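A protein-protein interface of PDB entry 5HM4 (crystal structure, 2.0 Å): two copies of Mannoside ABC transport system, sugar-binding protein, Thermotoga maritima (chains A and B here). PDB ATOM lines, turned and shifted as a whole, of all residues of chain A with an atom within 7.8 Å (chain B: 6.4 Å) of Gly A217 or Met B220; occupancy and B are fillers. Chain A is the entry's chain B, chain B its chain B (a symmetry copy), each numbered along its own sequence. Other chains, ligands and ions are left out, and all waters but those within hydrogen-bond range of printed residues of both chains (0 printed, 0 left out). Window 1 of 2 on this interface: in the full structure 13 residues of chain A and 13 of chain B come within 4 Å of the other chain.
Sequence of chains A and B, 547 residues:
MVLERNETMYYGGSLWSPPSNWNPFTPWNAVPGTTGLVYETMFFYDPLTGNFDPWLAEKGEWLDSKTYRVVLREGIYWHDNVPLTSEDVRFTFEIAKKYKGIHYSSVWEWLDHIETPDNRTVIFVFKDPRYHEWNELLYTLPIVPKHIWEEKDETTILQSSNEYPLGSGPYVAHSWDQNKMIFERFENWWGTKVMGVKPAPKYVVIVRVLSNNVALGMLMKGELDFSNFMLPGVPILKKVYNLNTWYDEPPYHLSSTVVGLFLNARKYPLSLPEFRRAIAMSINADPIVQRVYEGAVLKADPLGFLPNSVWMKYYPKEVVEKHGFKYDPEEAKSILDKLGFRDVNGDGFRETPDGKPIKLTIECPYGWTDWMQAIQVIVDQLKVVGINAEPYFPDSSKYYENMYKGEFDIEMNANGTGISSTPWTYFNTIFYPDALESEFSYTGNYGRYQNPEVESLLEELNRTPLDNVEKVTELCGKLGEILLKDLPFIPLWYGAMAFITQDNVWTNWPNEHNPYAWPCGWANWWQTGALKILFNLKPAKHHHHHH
Ala A215 touches none of the printed residues of chain B.
Of the printed residues of chain B, Gly A217 touches Gly B217, Met B220 and Lys B221.
Of the printed residues of chain B, Met A220 touches Asn B213 (3.4 Å) and Gly B217 (3.7 Å).
Of the printed residues of chain B, Glu A223 touches Lys B221.
Of the printed residues of chain A, Leu B216 touches Tyr A241.
Printed residues of chain A within 4 Å of Met B220: Asn A213 (3.4 Å) and Gly A217 (3.7 Å).
Hydrophobic or aromatic side chains of chain A within 4 Å of the printed part of chain B: Leu A216, Met A218, Met A220, Leu A231 and Tyr A241.
Hydrophobic or aromatic side chains of chain B that line the printed part of chain A: Leu B216, Met B218, Met B220 and Tyr B241.
Among the printed residues, Asp or Glu carboxylates within 4 Å of a Lys or Arg side-chain nitrogen of the other chain: Lys A221 with Glu B223 (2.7 Å) and Glu A223 with Lys B221 (2.7 Å).
The backbone NH (N) of Glu A223 is in hydrogen-bond range of the backbone carbonyl oxygen (O) of Met A218, 2.7 Å away.
N of Glu B223 lies within hydrogen-bond range of O of Met B218 (2.7 Å).
The backbone carbonyl oxygen (O) of Met A218 sits at hydrogen-bond distance from the backbone NH (N) of Leu A224, 3.3 Å away.
The side-chain carboxylate (OE2) of Glu A223 is in salt-bridge range of the side-chain amino group (NZ) of Lys A221 (2.6 Å).
The side-chain hydroxyl of Ser A211 lies close to the backbone NH of Val A214.
NZ of Lys B221 lies within salt-bridge range of OE2 of Glu B223, at 2.6 Å.
Asn A213 touches Tyr B241, and with the chains exchanged Tyr A241 touches Asn B213.
Gly A217 touches its own counterpart, Gly B217.
Gly A217 touches Lys B221, and with the chains exchanged Lys A221 touches Gly B217.
Met A218 touches Lys B221, and with the chains exchanged Lys A221 touches Met B218.
14 positions are printed for both chains.
Among the printed residues, merely in contact across the chains: Met A220 with Asn B213, Asn A213 with Met B220, Leu A216 with Tyr B241, Tyr A241 with Leu B216, Gly A217 with Gly B217, Gly A217 with Met B220, Met A220 with Gly B217, Lys A221 with Lys B221, Met A218 with Lys B221, Lys A221 with Met B218, Leu A231 with Tyr B241, Lys A221 with Gly B217, Gly A217 with Lys B221, Val A214 with Lys B221 and Lys A221 with Val B214.
NZ of Lys B221 lies within salt-bridge range of OE1 of Glu A223 (2.7 Å).
The side-chain amide nitrogen of Asn A213 sits at hydrogen-bond distance from the backbone carbonyl oxygen of Tyr B241.
The side-chain carboxylate (OE1) of Glu B223 lies within salt-bridge range of the side-chain amino group (NZ) of Lys A221, 2.7 Å away.
The backbone carbonyl oxygen (O) of Tyr A241 sits at hydrogen-bond distance from the side-chain amide nitrogen (ND2) of Asn B213, at 2.8 Å.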
ATOM      1  N   SER A 211      26.134 -12.379 -26.213  1.00  0.00           N
ATOM      2  CA  SER A 211      25.529 -11.575 -27.264  1.00  0.00           C
ATOM      3  C   SER A 211      24.083 -11.249 -26.917  1.00  0.00           C
ATOM      4  O   SER A 211      23.443 -11.934 -26.114  1.00  0.00           O
ATOM      5  CB  SER A 211      25.595 -12.291 -28.616  1.00  0.00           C
ATOM      6  OG  SER A 211      24.767 -13.437 -28.620  1.00  0.00           O
ATOM      7  N   ASN A 212      23.572 -10.191 -27.558  1.00  0.00           N
ATOM      8  CA  ASN A 212      22.175  -9.808 -27.385  1.00  0.00           C
ATOM      9  C   ASN A 212      21.227 -10.839 -27.986  1.00  0.00           C
ATOM     10  O   ASN A 212      20.079 -10.952 -27.540  1.00  0.00           O
ATOM     11  CB  ASN A 212      21.927  -8.431 -28.002  1.00  0.00           C
ATOM     12  CG  ASN A 212      22.485  -7.301 -27.154  1.00  0.00           C
ATOM     13  OD1 ASN A 212      22.774  -7.486 -25.973  1.00  0.00           O
ATOM     14  ND2 ASN A 212      22.631  -6.121 -27.751  1.00  0.00           N
ATOM     15  N   ASN A 213      21.680 -11.586 -28.999  1.00  0.00           N
ATOM     16  CA  ASN A 213      20.897 -12.706 -29.512  1.00  0.00           C
ATOM     17  C   ASN A 213      20.537 -13.674 -28.392  1.00  0.00           C
ATOM     18  O   ASN A 213      19.371 -14.042 -28.217  1.00  0.00           O
ATOM     19  CB  ASN A 213      21.680 -13.439 -30.607  1.00  0.00           C
ATOM     20  CG  ASN A 213      21.516 -12.807 -31.975  1.00  0.00           C
ATOM     21  OD1 ASN A 213      21.929 -11.671 -32.202  1.00  0.00           O
ATOM     22  ND2 ASN A 213      20.924 -13.551 -32.902  1.00  0.00           N
ATOM     23  N   VAL A 214      21.543 -14.089 -27.621  1.00  0.00           N
ATOM     24  CA  VAL A 214      21.325 -15.045 -26.538  1.00  0.00           C
ATOM     25  C   VAL A 214      20.411 -14.462 -25.474  1.00  0.00           C
ATOM     26  O   VAL A 214      19.521 -15.148 -24.956  1.00  0.00           O
ATOM     27  CB  VAL A 214      22.680 -15.471 -25.946  1.00  0.00           C
ATOM     28  CG1 VAL A 214      22.486 -16.519 -24.853  1.00  0.00           C
ATOM     29  CG2 VAL A 214      23.610 -15.983 -27.056  1.00  0.00           C
ATOM     30  N   ALA A 215      20.599 -13.187 -25.133  1.00  0.00           N
ATOM     31  CA  ALA A 215      19.797 -12.569 -24.085  1.00  0.00           C
ATOM     32  C   ALA A 215      18.333 -12.473 -24.496  1.00  0.00           C
ATOM     33  O   ALA A 215      17.433 -12.804 -23.716  1.00  0.00           O
ATOM     34  CB  ALA A 215      20.356 -11.189 -23.744  1.00  0.00           C
ATOM     35  N   LEU A 216      18.074 -12.018 -25.726  1.00  0.00           N
ATOM     36  CA  LEU A 216      16.695 -11.943 -26.195  1.00  0.00           C
ATOM     37  C   LEU A 216      16.081 -13.332 -26.308  1.00  0.00           C
ATOM     38  O   LEU A 216      14.912 -13.530 -25.961  1.00  0.00           O
ATOM     39  CB  LEU A 216      16.625 -11.209 -27.533  1.00  0.00           C
ATOM     40  CG  LEU A 216      15.202 -10.997 -28.054  1.00  0.00           C
ATOM     41  CD1 LEU A 216      14.313 -10.390 -26.984  1.00  0.00           C
ATOM     42  CD2 LEU A 216      15.188 -10.128 -29.296  1.00  0.00           C
ATOM     43  N   GLY A 217      16.861 -14.309 -26.774  1.00  0.00           N
ATOM     44  CA  GLY A 217      16.360 -15.672 -26.837  1.00  0.00           C
ATOM     45  C   GLY A 217      15.937 -16.202 -25.481  1.00  0.00           C
ATOM     46  O   GLY A 217      14.921 -16.892 -25.364  1.00  0.00           O
ATOM     47  N   MET A 218      16.702 -15.877 -24.435  1.00  0.00           N
ATOM     48  CA  MET A 218      16.356 -16.342 -23.095  1.00  0.00           C
ATOM     49  C   MET A 218      15.058 -15.711 -22.608  1.00  0.00           C
ATOM     50  O   MET A 218      14.219 -16.392 -22.009  1.00  0.00           O
ATOM     51  CB  MET A 218      17.498 -16.050 -22.121  1.00  0.00           C
ATOM     52  CG  MET A 218      18.729 -16.924 -22.332  1.00  0.00           C
ATOM     53  SD  MET A 218      20.081 -16.556 -21.195  1.00  0.00           S
ATOM     54  CE  MET A 218      19.696 -17.650 -19.828  1.00  0.00           C
ATOM     55  N   LEU A 219      14.876 -14.409 -22.851  1.00  0.00           N
ATOM     56  CA  LEU A 219      13.611 -13.765 -22.507  1.00  0.00           C
ATOM     57  C   LEU A 219      12.445 -14.422 -23.240  1.00  0.00           C
ATOM     58  O   LEU A 219      11.407 -14.718 -22.637  1.00  0.00           O
ATOM     59  CB  LEU A 219      13.668 -12.271 -22.825  1.00  0.00           C
ATOM     60  CG  LEU A 219      14.429 -11.322 -21.897  1.00  0.00           C
ATOM     61  CD1 LEU A 219      14.713 -10.010 -22.611  1.00  0.00           C
ATOM     62  CD2 LEU A 219      13.652 -11.071 -20.615  1.00  0.00           C
ATOM     63  N   MET A 220      12.602 -14.647 -24.549  1.00  0.00           N
ATOM     64  CA  MET A 220      11.555 -15.290 -25.339  1.00  0.00           C
ATOM     65  C   MET A 220      11.206 -16.661 -24.778  1.00  0.00           C
ATOM     66  O   MET A 220      10.028 -17.000 -24.619  1.00  0.00           O
ATOM     67  CB  MET A 220      12.003 -15.412 -26.796  1.00  0.00           C
ATOM     68  CG  MET A 220      12.130 -14.094 -27.535  1.00  0.00           C
ATOM     69  SD  MET A 220      10.535 -13.328 -27.858  1.00  0.00           S
ATOM     70  CE  MET A 220      11.055 -11.822 -28.676  1.00  0.00           C
ATOM     71  N   LYS A 221      12.224 -17.469 -24.477  1.00  0.00           N
ATOM     72  CA  LYS A 221      12.006 -18.800 -23.924  1.00  0.00           C
ATOM     73  C   LYS A 221      11.547 -18.769 -22.473  1.00  0.00           C
ATOM     74  O   LYS A 221      11.226 -19.828 -21.921  1.00  0.00           O
ATOM     75  CB  LYS A 221      13.282 -19.640 -24.029  1.00  0.00           C
ATOM     76  CG  LYS A 221      13.704 -19.987 -25.448  1.00  0.00           C
ATOM     77  CD  LYS A 221      14.921 -20.904 -25.445  1.00  0.00           C
ATOM     78  CE  LYS A 221      14.560 -22.315 -24.995  1.00  0.00           C
ATOM     79  NZ  LYS A 221      15.758 -23.091 -24.564  1.00  0.00           N
ATOM     80  N   GLY A 222      11.509 -17.594 -21.847  1.00  0.00           N
ATOM     81  CA  GLY A 222      11.175 -17.515 -20.440  1.00  0.00           C
ATOM     82  C   GLY A 222      12.279 -17.960 -19.511  1.00  0.00           C
ATOM     83  O   GLY A 222      12.005 -18.324 -18.367  1.00  0.00           O
ATOM     84  N   GLU A 223      13.527 -17.952 -19.977  1.00  0.00           N
ATOM     85  CA  GLU A 223      14.668 -18.347 -19.165  1.00  0.00           C
ATOM     86  C   GLU A 223      15.295 -17.177 -18.421  1.00  0.00           C
ATOM     87  O   GLU A 223      16.086 -17.400 -17.498  1.00  0.00           O
ATOM     88  CB  GLU A 223      15.727 -19.027 -20.042  1.00  0.00           C
ATOM     89  CG  GLU A 223      15.292 -20.380 -20.581  1.00  0.00           C
ATOM     90  CD  GLU A 223      16.126 -20.829 -21.739  1.00  0.00           C
ATOM     91  OE1 GLU A 223      17.027 -20.070 -22.167  1.00  0.00           O
ATOM     92  OE2 GLU A 223      15.900 -21.961 -22.225  1.00  0.00           O
ATOM     93  N   LEU A 224      14.966 -15.948 -18.808  1.00  0.00           N
ATOM     94  CA  LEU A 224      15.439 -14.734 -18.159  1.00  0.00           C
ATOM     95  C   LEU A 224      14.220 -13.980 -17.649  1.00  0.00           C
ATOM     96  O   LEU A 224      13.241 -13.811 -18.383  1.00  0.00           O
ATOM     97  CB  LEU A 224      16.246 -13.879 -19.144  1.00  0.00           C
ATOM     98  CG  LEU A 224      17.406 -12.969 -18.721  1.00  0.00           C
ATOM     99  CD1 LEU A 224      18.331 -13.655 -17.736  1.00  0.00           C
ATOM    100  CD2 LEU A 224      18.178 -12.552 -19.962  1.00  0.00           C
ATOM    101  N   LEU A 231      18.564  -4.176 -25.857  1.00  0.00           N
ATOM    102  CA  LEU A 231      18.060  -5.010 -26.934  1.00  0.00           C
ATOM    103  C   LEU A 231      17.281  -4.176 -27.937  1.00  0.00           C
ATOM    104  O   LEU A 231      16.215  -3.644 -27.593  1.00  0.00           O
ATOM    105  CB  LEU A 231      17.181  -6.126 -26.378  1.00  0.00           C
ATOM    106  CG  LEU A 231      17.860  -7.115 -25.433  1.00  0.00           C
ATOM    107  CD1 LEU A 231      16.834  -8.068 -24.852  1.00  0.00           C
ATOM    108  CD2 LEU A 231      18.955  -7.880 -26.155  1.00  0.00           C
ATOM    109  N   TYR A 241       5.379 -10.362 -28.981  1.00  0.00           N
ATOM    110  CA  TYR A 241       6.037 -11.442 -28.254  1.00  0.00           C
ATOM    111  C   TYR A 241       5.913 -11.322 -26.738  1.00  0.00           C
ATOM    112  O   TYR A 241       6.663 -11.984 -26.014  1.00  0.00           O
ATOM    113  CB  TYR A 241       7.505 -11.537 -28.671  1.00  0.00           C
ATOM    114  CG  TYR A 241       7.665 -12.109 -30.059  1.00  0.00           C
ATOM    115  CD1 TYR A 241       7.717 -13.481 -30.260  1.00  0.00           C
ATOM    116  CD2 TYR A 241       7.738 -11.279 -31.170  1.00  0.00           C
ATOM    117  CE1 TYR A 241       7.850 -14.013 -31.526  1.00  0.00           C
ATOM    118  CE2 TYR A 241       7.873 -11.803 -32.443  1.00  0.00           C
ATOM    119  CZ  TYR A 241       7.927 -13.170 -32.615  1.00  0.00           C
ATOM    120  OH  TYR A 241       8.063 -13.697 -33.878  1.00  0.00           O
ATOM    121  N   LEU A 243       6.621  -9.237 -24.365  1.00  0.00           N
ATOM    122  CA  LEU A 243       7.699  -8.704 -23.544  1.00  0.00           C
ATOM    123  C   LEU A 243       7.300  -7.323 -23.045  1.00  0.00           C
ATOM    124  O   LEU A 243       6.734  -6.522 -23.793  1.00  0.00           O
ATOM    125  CB  LEU A 243       9.009  -8.619 -24.325  1.00  0.00           C
ATOM    126  CG  LEU A 243       9.556  -9.904 -24.944  1.00  0.00           C
ATOM    127  CD1 LEU A 243      10.944  -9.657 -25.506  1.00  0.00           C
ATOM    128  CD2 LEU A 243       9.581 -11.026 -23.925  1.00  0.00           C
ATOM    129  N   ASN B 213       6.995 -17.934 -29.168  1.00  0.00           N
ATOM    130  CA  ASN B 213       8.005 -17.348 -28.291  1.00  0.00           C
ATOM    131  C   ASN B 213       9.179 -18.300 -28.105  1.00  0.00           C
ATOM    132  O   ASN B 213      10.341 -17.922 -28.287  1.00  0.00           O
ATOM    133  CB  ASN B 213       7.387 -17.005 -26.931  1.00  0.00           C
ATOM    134  CG  ASN B 213       6.707 -15.650 -26.915  1.00  0.00           C
ATOM    135  OD1 ASN B 213       5.718 -15.429 -27.612  1.00  0.00           O
ATOM    136  ND2 ASN B 213       7.228 -14.738 -26.103  1.00  0.00           N
ATOM    137  N   VAL B 214       8.879 -19.548 -27.744  1.00  0.00           N
ATOM    138  CA  VAL B 214       9.924 -20.540 -27.502  1.00  0.00           C
ATOM    139  C   VAL B 214      10.710 -20.823 -28.771  1.00  0.00           C
ATOM    140  O   VAL B 214      11.942 -20.940 -28.742  1.00  0.00           O
ATOM    141  CB  VAL B 214       9.294 -21.823 -26.931  1.00  0.00           C
ATOM    142  CG1 VAL B 214      10.372 -22.856 -26.608  1.00  0.00           C
ATOM    143  CG2 VAL B 214       8.443 -21.495 -25.695  1.00  0.00           C
ATOM    144  N   ALA B 215      10.026 -20.925 -29.909  1.00  0.00           N
ATOM    145  CA  ALA B 215      10.701 -21.245 -31.160  1.00  0.00           C
ATOM    146  C   ALA B 215      11.649 -20.128 -31.575  1.00  0.00           C
ATOM    147  O   ALA B 215      12.798 -20.380 -31.958  1.00  0.00           O
ATOM    148  CB  ALA B 215       9.671 -21.516 -32.255  1.00  0.00           C
ATOM    149  N   LEU B 216      11.184 -18.876 -31.507  1.00  0.00           N
ATOM    150  CA  LEU B 216      12.057 -17.759 -31.849  1.00  0.00           C
ATOM    151  C   LEU B 216      13.214 -17.649 -30.865  1.00  0.00           C
ATOM    152  O   LEU B 216      14.352 -17.376 -31.263  1.00  0.00           O
ATOM    153  CB  LEU B 216      11.262 -16.455 -31.897  1.00  0.00           C
ATOM    154  CG  LEU B 216      12.080 -15.243 -32.346  1.00  0.00           C
ATOM    155  CD1 LEU B 216      12.837 -15.538 -33.628  1.00  0.00           C
ATOM    156  CD2 LEU B 216      11.206 -14.018 -32.528  1.00  0.00           C
ATOM    157  N   GLY B 217      12.946 -17.878 -29.578  1.00  0.00           N
ATOM    158  CA  GLY B 217      14.020 -17.864 -28.598  1.00  0.00           C
ATOM    159  C   GLY B 217      15.100 -18.883 -28.899  1.00  0.00           C
ATOM    160  O   GLY B 217      16.290 -18.605 -28.736  1.00  0.00           O
ATOM    161  N   MET B 218      14.703 -20.074 -29.356  1.00  0.00           N
ATOM    162  CA  MET B 218      15.684 -21.106 -29.677  1.00  0.00           C
ATOM    163  C   MET B 218      16.542 -20.702 -30.869  1.00  0.00           C
ATOM    164  O   MET B 218      17.761 -20.913 -30.861  1.00  0.00           O
ATOM    165  CB  MET B 218      14.984 -22.439 -29.943  1.00  0.00           C
ATOM    166  CG  MET B 218      14.401 -23.091 -28.694  1.00  0.00           C
ATOM    167  SD  MET B 218      13.555 -24.651 -29.020  1.00  0.00           S
ATOM    168  CE  MET B 218      14.901 -25.821 -28.846  1.00  0.00           C
ATOM    169  N   LEU B 219      15.927 -20.124 -31.905  1.00  0.00           N
ATOM    170  CA  LEU B 219      16.703 -19.616 -33.033  1.00  0.00           C
ATOM    171  C   LEU B 219      17.694 -18.549 -32.579  1.00  0.00           C
ATOM    172  O   LEU B 219      18.870 -18.576 -32.962  1.00  0.00           O
ATOM    173  CB  LEU B 219      15.774 -19.057 -34.112  1.00  0.00           C
ATOM    174  CG  LEU B 219      15.016 -20.012 -35.035  1.00  0.00           C
ATOM    175  CD1 LEU B 219      13.866 -19.283 -35.711  1.00  0.00           C
ATOM    176  CD2 LEU B 219      15.943 -20.619 -36.076  1.00  0.00           C
ATOM    177  N   MET B 220      17.228 -17.595 -31.766  1.00  0.00           N
ATOM    178  CA  MET B 220      18.100 -16.539 -31.257  1.00  0.00           C
ATOM    179  C   MET B 220      19.278 -17.121 -30.489  1.00  0.00           C
ATOM    180  O   MET B 220      20.429 -16.718 -30.691  1.00  0.00           O
ATOM    181  CB  MET B 220      17.301 -15.590 -30.363  1.00  0.00           C
ATOM    182  CG  MET B 220      16.262 -14.757 -31.087  1.00  0.00           C
ATOM    183  SD  MET B 220      16.997 -13.499 -32.142  1.00  0.00           S
ATOM    184  CE  MET B 220      15.525 -12.764 -32.848  1.00  0.00           C
ATOM    185  N   LYS B 221      19.006 -18.071 -29.593  1.00  0.00           N
ATOM    186  CA  LYS B 221      20.059 -18.706 -28.809  1.00  0.00           C
ATOM    187  C   LYS B 221      20.911 -19.664 -29.630  1.00  0.00           C
ATOM    188  O   LYS B 221      21.903 -20.185 -29.105  1.00  0.00           O
ATOM    189  CB  LYS B 221      19.459 -19.461 -27.619  1.00  0.00           C
ATOM    190  CG  LYS B 221      18.811 -18.579 -26.564  1.00  0.00           C
ATOM    191  CD  LYS B 221      18.335 -19.409 -25.378  1.00  0.00           C
ATOM    192  CE  LYS B 221      19.505 -19.901 -24.532  1.00  0.00           C
ATOM    193  NZ  LYS B 221      19.121 -21.046 -23.657  1.00  0.00           N
ATOM    194  N   GLY B 222      20.554 -19.907 -30.889  1.00  0.00           N
ATOM    195  CA  GLY B 222      21.268 -20.883 -31.686  1.00  0.00           C
ATOM    196  C   GLY B 222      20.963 -22.320 -31.334  1.00  0.00           C
ATOM    197  O   GLY B 222      21.767 -23.205 -31.629  1.00  0.00           O
ATOM    198  N   GLU B 223      19.821 -22.576 -30.699  1.00  0.00           N
ATOM    199  CA  GLU B 223      19.420 -23.924 -30.326  1.00  0.00           C
ATOM    200  C   GLU B 223      18.587 -24.610 -31.398  1.00  0.00           C
ATOM    201  O   GLU B 223      18.409 -25.832 -31.338  1.00  0.00           O
ATOM    202  CB  GLU B 223      18.636 -23.893 -29.007  1.00  0.00           C
ATOM    203  CG  GLU B 223      19.484 -23.515 -27.804  1.00  0.00           C
ATOM    204  CD  GLU B 223      18.659 -23.085 -26.634  1.00  0.00           C
ATOM    205  OE1 GLU B 223      17.413 -23.031 -26.758  1.00  0.00           O
ATOM    206  OE2 GLU B 223      19.249 -22.811 -25.564  1.00  0.00           O
ATOM    207  N   LEU B 224      18.073 -23.853 -32.363  1.00  0.00           N
ATOM    208  CA  LEU B 224      17.305 -24.371 -33.486  1.00  0.00           C
ATOM    209  C   LEU B 224      18.046 -24.000 -34.761  1.00  0.00           C
ATOM    210  O   LEU B 224      18.465 -22.850 -34.925  1.00  0.00           O
ATOM    211  CB  LEU B 224      15.886 -23.787 -33.480  1.00  0.00           C
ATOM    212  CG  LEU B 224      14.660 -24.538 -34.011  1.00  0.00           C
ATOM    213  CD1 LEU B 224      14.638 -25.982 -33.547  1.00  0.00           C
ATOM    214  CD2 LEU B 224      13.405 -23.820 -33.543  1.00  0.00           C
ATOM    215  N   LEU B 237      13.936  -9.036 -37.379  1.00  0.00           N
ATOM    216  CA  LEU B 237      14.792 -10.173 -37.055  1.00  0.00           C
ATOM    217  C   LEU B 237      16.006 -10.216 -37.974  1.00  0.00           C
ATOM    218  O   LEU B 237      17.150 -10.266 -37.507  1.00  0.00           O
ATOM    219  CB  LEU B 237      13.994 -11.473 -37.150  1.00  0.00           C
ATOM    220  N   TYR B 241      19.095  -9.261 -35.921  1.00  0.00           N
ATOM    221  CA  TYR B 241      19.395 -10.439 -35.112  1.00  0.00           C
ATOM    222  C   TYR B 241      19.963 -11.603 -35.916  1.00  0.00           C
ATOM    223  O   TYR B 241      19.974 -12.734 -35.420  1.00  0.00           O
ATOM    224  CB  TYR B 241      18.152 -10.872 -34.335  1.00  0.00           C
ATOM    225  CG  TYR B 241      17.834  -9.929 -33.200  1.00  0.00           C
ATOM    226  CD1 TYR B 241      18.431 -10.088 -31.957  1.00  0.00           C
ATOM    227  CD2 TYR B 241      16.958  -8.866 -33.376  1.00  0.00           C
ATOM    228  CE1 TYR B 241      18.157  -9.223 -30.917  1.00  0.00           C
ATOM    229  CE2 TYR B 241      16.675  -7.995 -32.339  1.00  0.00           C
ATOM    230  CZ  TYR B 241      17.279  -8.178 -31.113  1.00  0.00           C
ATOM    231  OH  TYR B 241      17.001  -7.316 -30.078  1.00  0.00           O
ATOM    232  N   LEU B 243      19.167 -13.483 -38.430  1.00  0.00           N
ATOM    233  CA  LEU B 243      18.339 -14.603 -38.851  1.00  0.00           C
ATOM    234  C   LEU B 243      18.112 -14.511 -40.352  1.00  0.00           C
ATOM    235  O   LEU B 243      17.877 -13.424 -40.889  1.00  0.00           O
ATOM    236  CB  LEU B 243      16.997 -14.615 -38.120  1.00  0.00           C
ATOM    237  CG  LEU B 243      17.017 -14.663 -36.593  1.00  0.00           C
ATOM    238  CD1 LEU B 243      15.608 -14.862 -36.064  1.00  0.00           C
ATOM    239  CD2 LEU B 243      17.935 -15.764 -36.099  1.00  0.00           C
ATOM    240  N   GLN B 502      19.764 -20.283 -38.975  1.00  0.00           N
ATOM    241  CA  GLN B 502      20.919 -19.578 -38.445  1.00  0.00           C
ATOM    242  C   GLN B 502      22.131 -20.487 -38.604  1.00  0.00           C
ATOM    243  O   GLN B 502      22.002 -21.713 -38.647  1.00  0.00           O
ATOM    244  CB  GLN B 502      20.695 -19.153 -36.986  1.00  0.00           C
ATOM    245  CG  GLN B 502      20.325 -20.279 -36.046  1.00  0.00           C
ATOM    246  CD  GLN B 502      21.540 -21.027 -35.558  1.00  0.00           C
ATOM    247  OE1 GLN B 502      22.656 -20.517 -35.632  1.00  0.00           O
ATOM    248  NE2 GLN B 502      21.336 -22.244 -35.071  1.00  0.00           N
ATOM    249  N   ASN B 504      25.184 -20.949 -36.904  1.00  0.00           N
ATOM    250  CA  ASN B 504      26.211 -21.140 -35.887  1.00  0.00           C
ATOM    251  C   ASN B 504      26.764 -22.561 -35.865  1.00  0.00           C
ATOM    252  O   ASN B 504      27.903 -22.754 -35.428  1.00  0.00           O
ATOM    253  CB  ASN B 504      25.667 -20.751 -34.512  1.00  0.00           C
ATOM    254  CG  ASN B 504      25.289 -19.283 -34.434  1.00  0.00           C
ATOM    255  OD1 ASN B 504      26.153 -18.412 -34.342  1.00  0.00           O
ATOM    256  ND2 ASN B 504      23.991 -19.001 -34.474  1.00  0.00           N
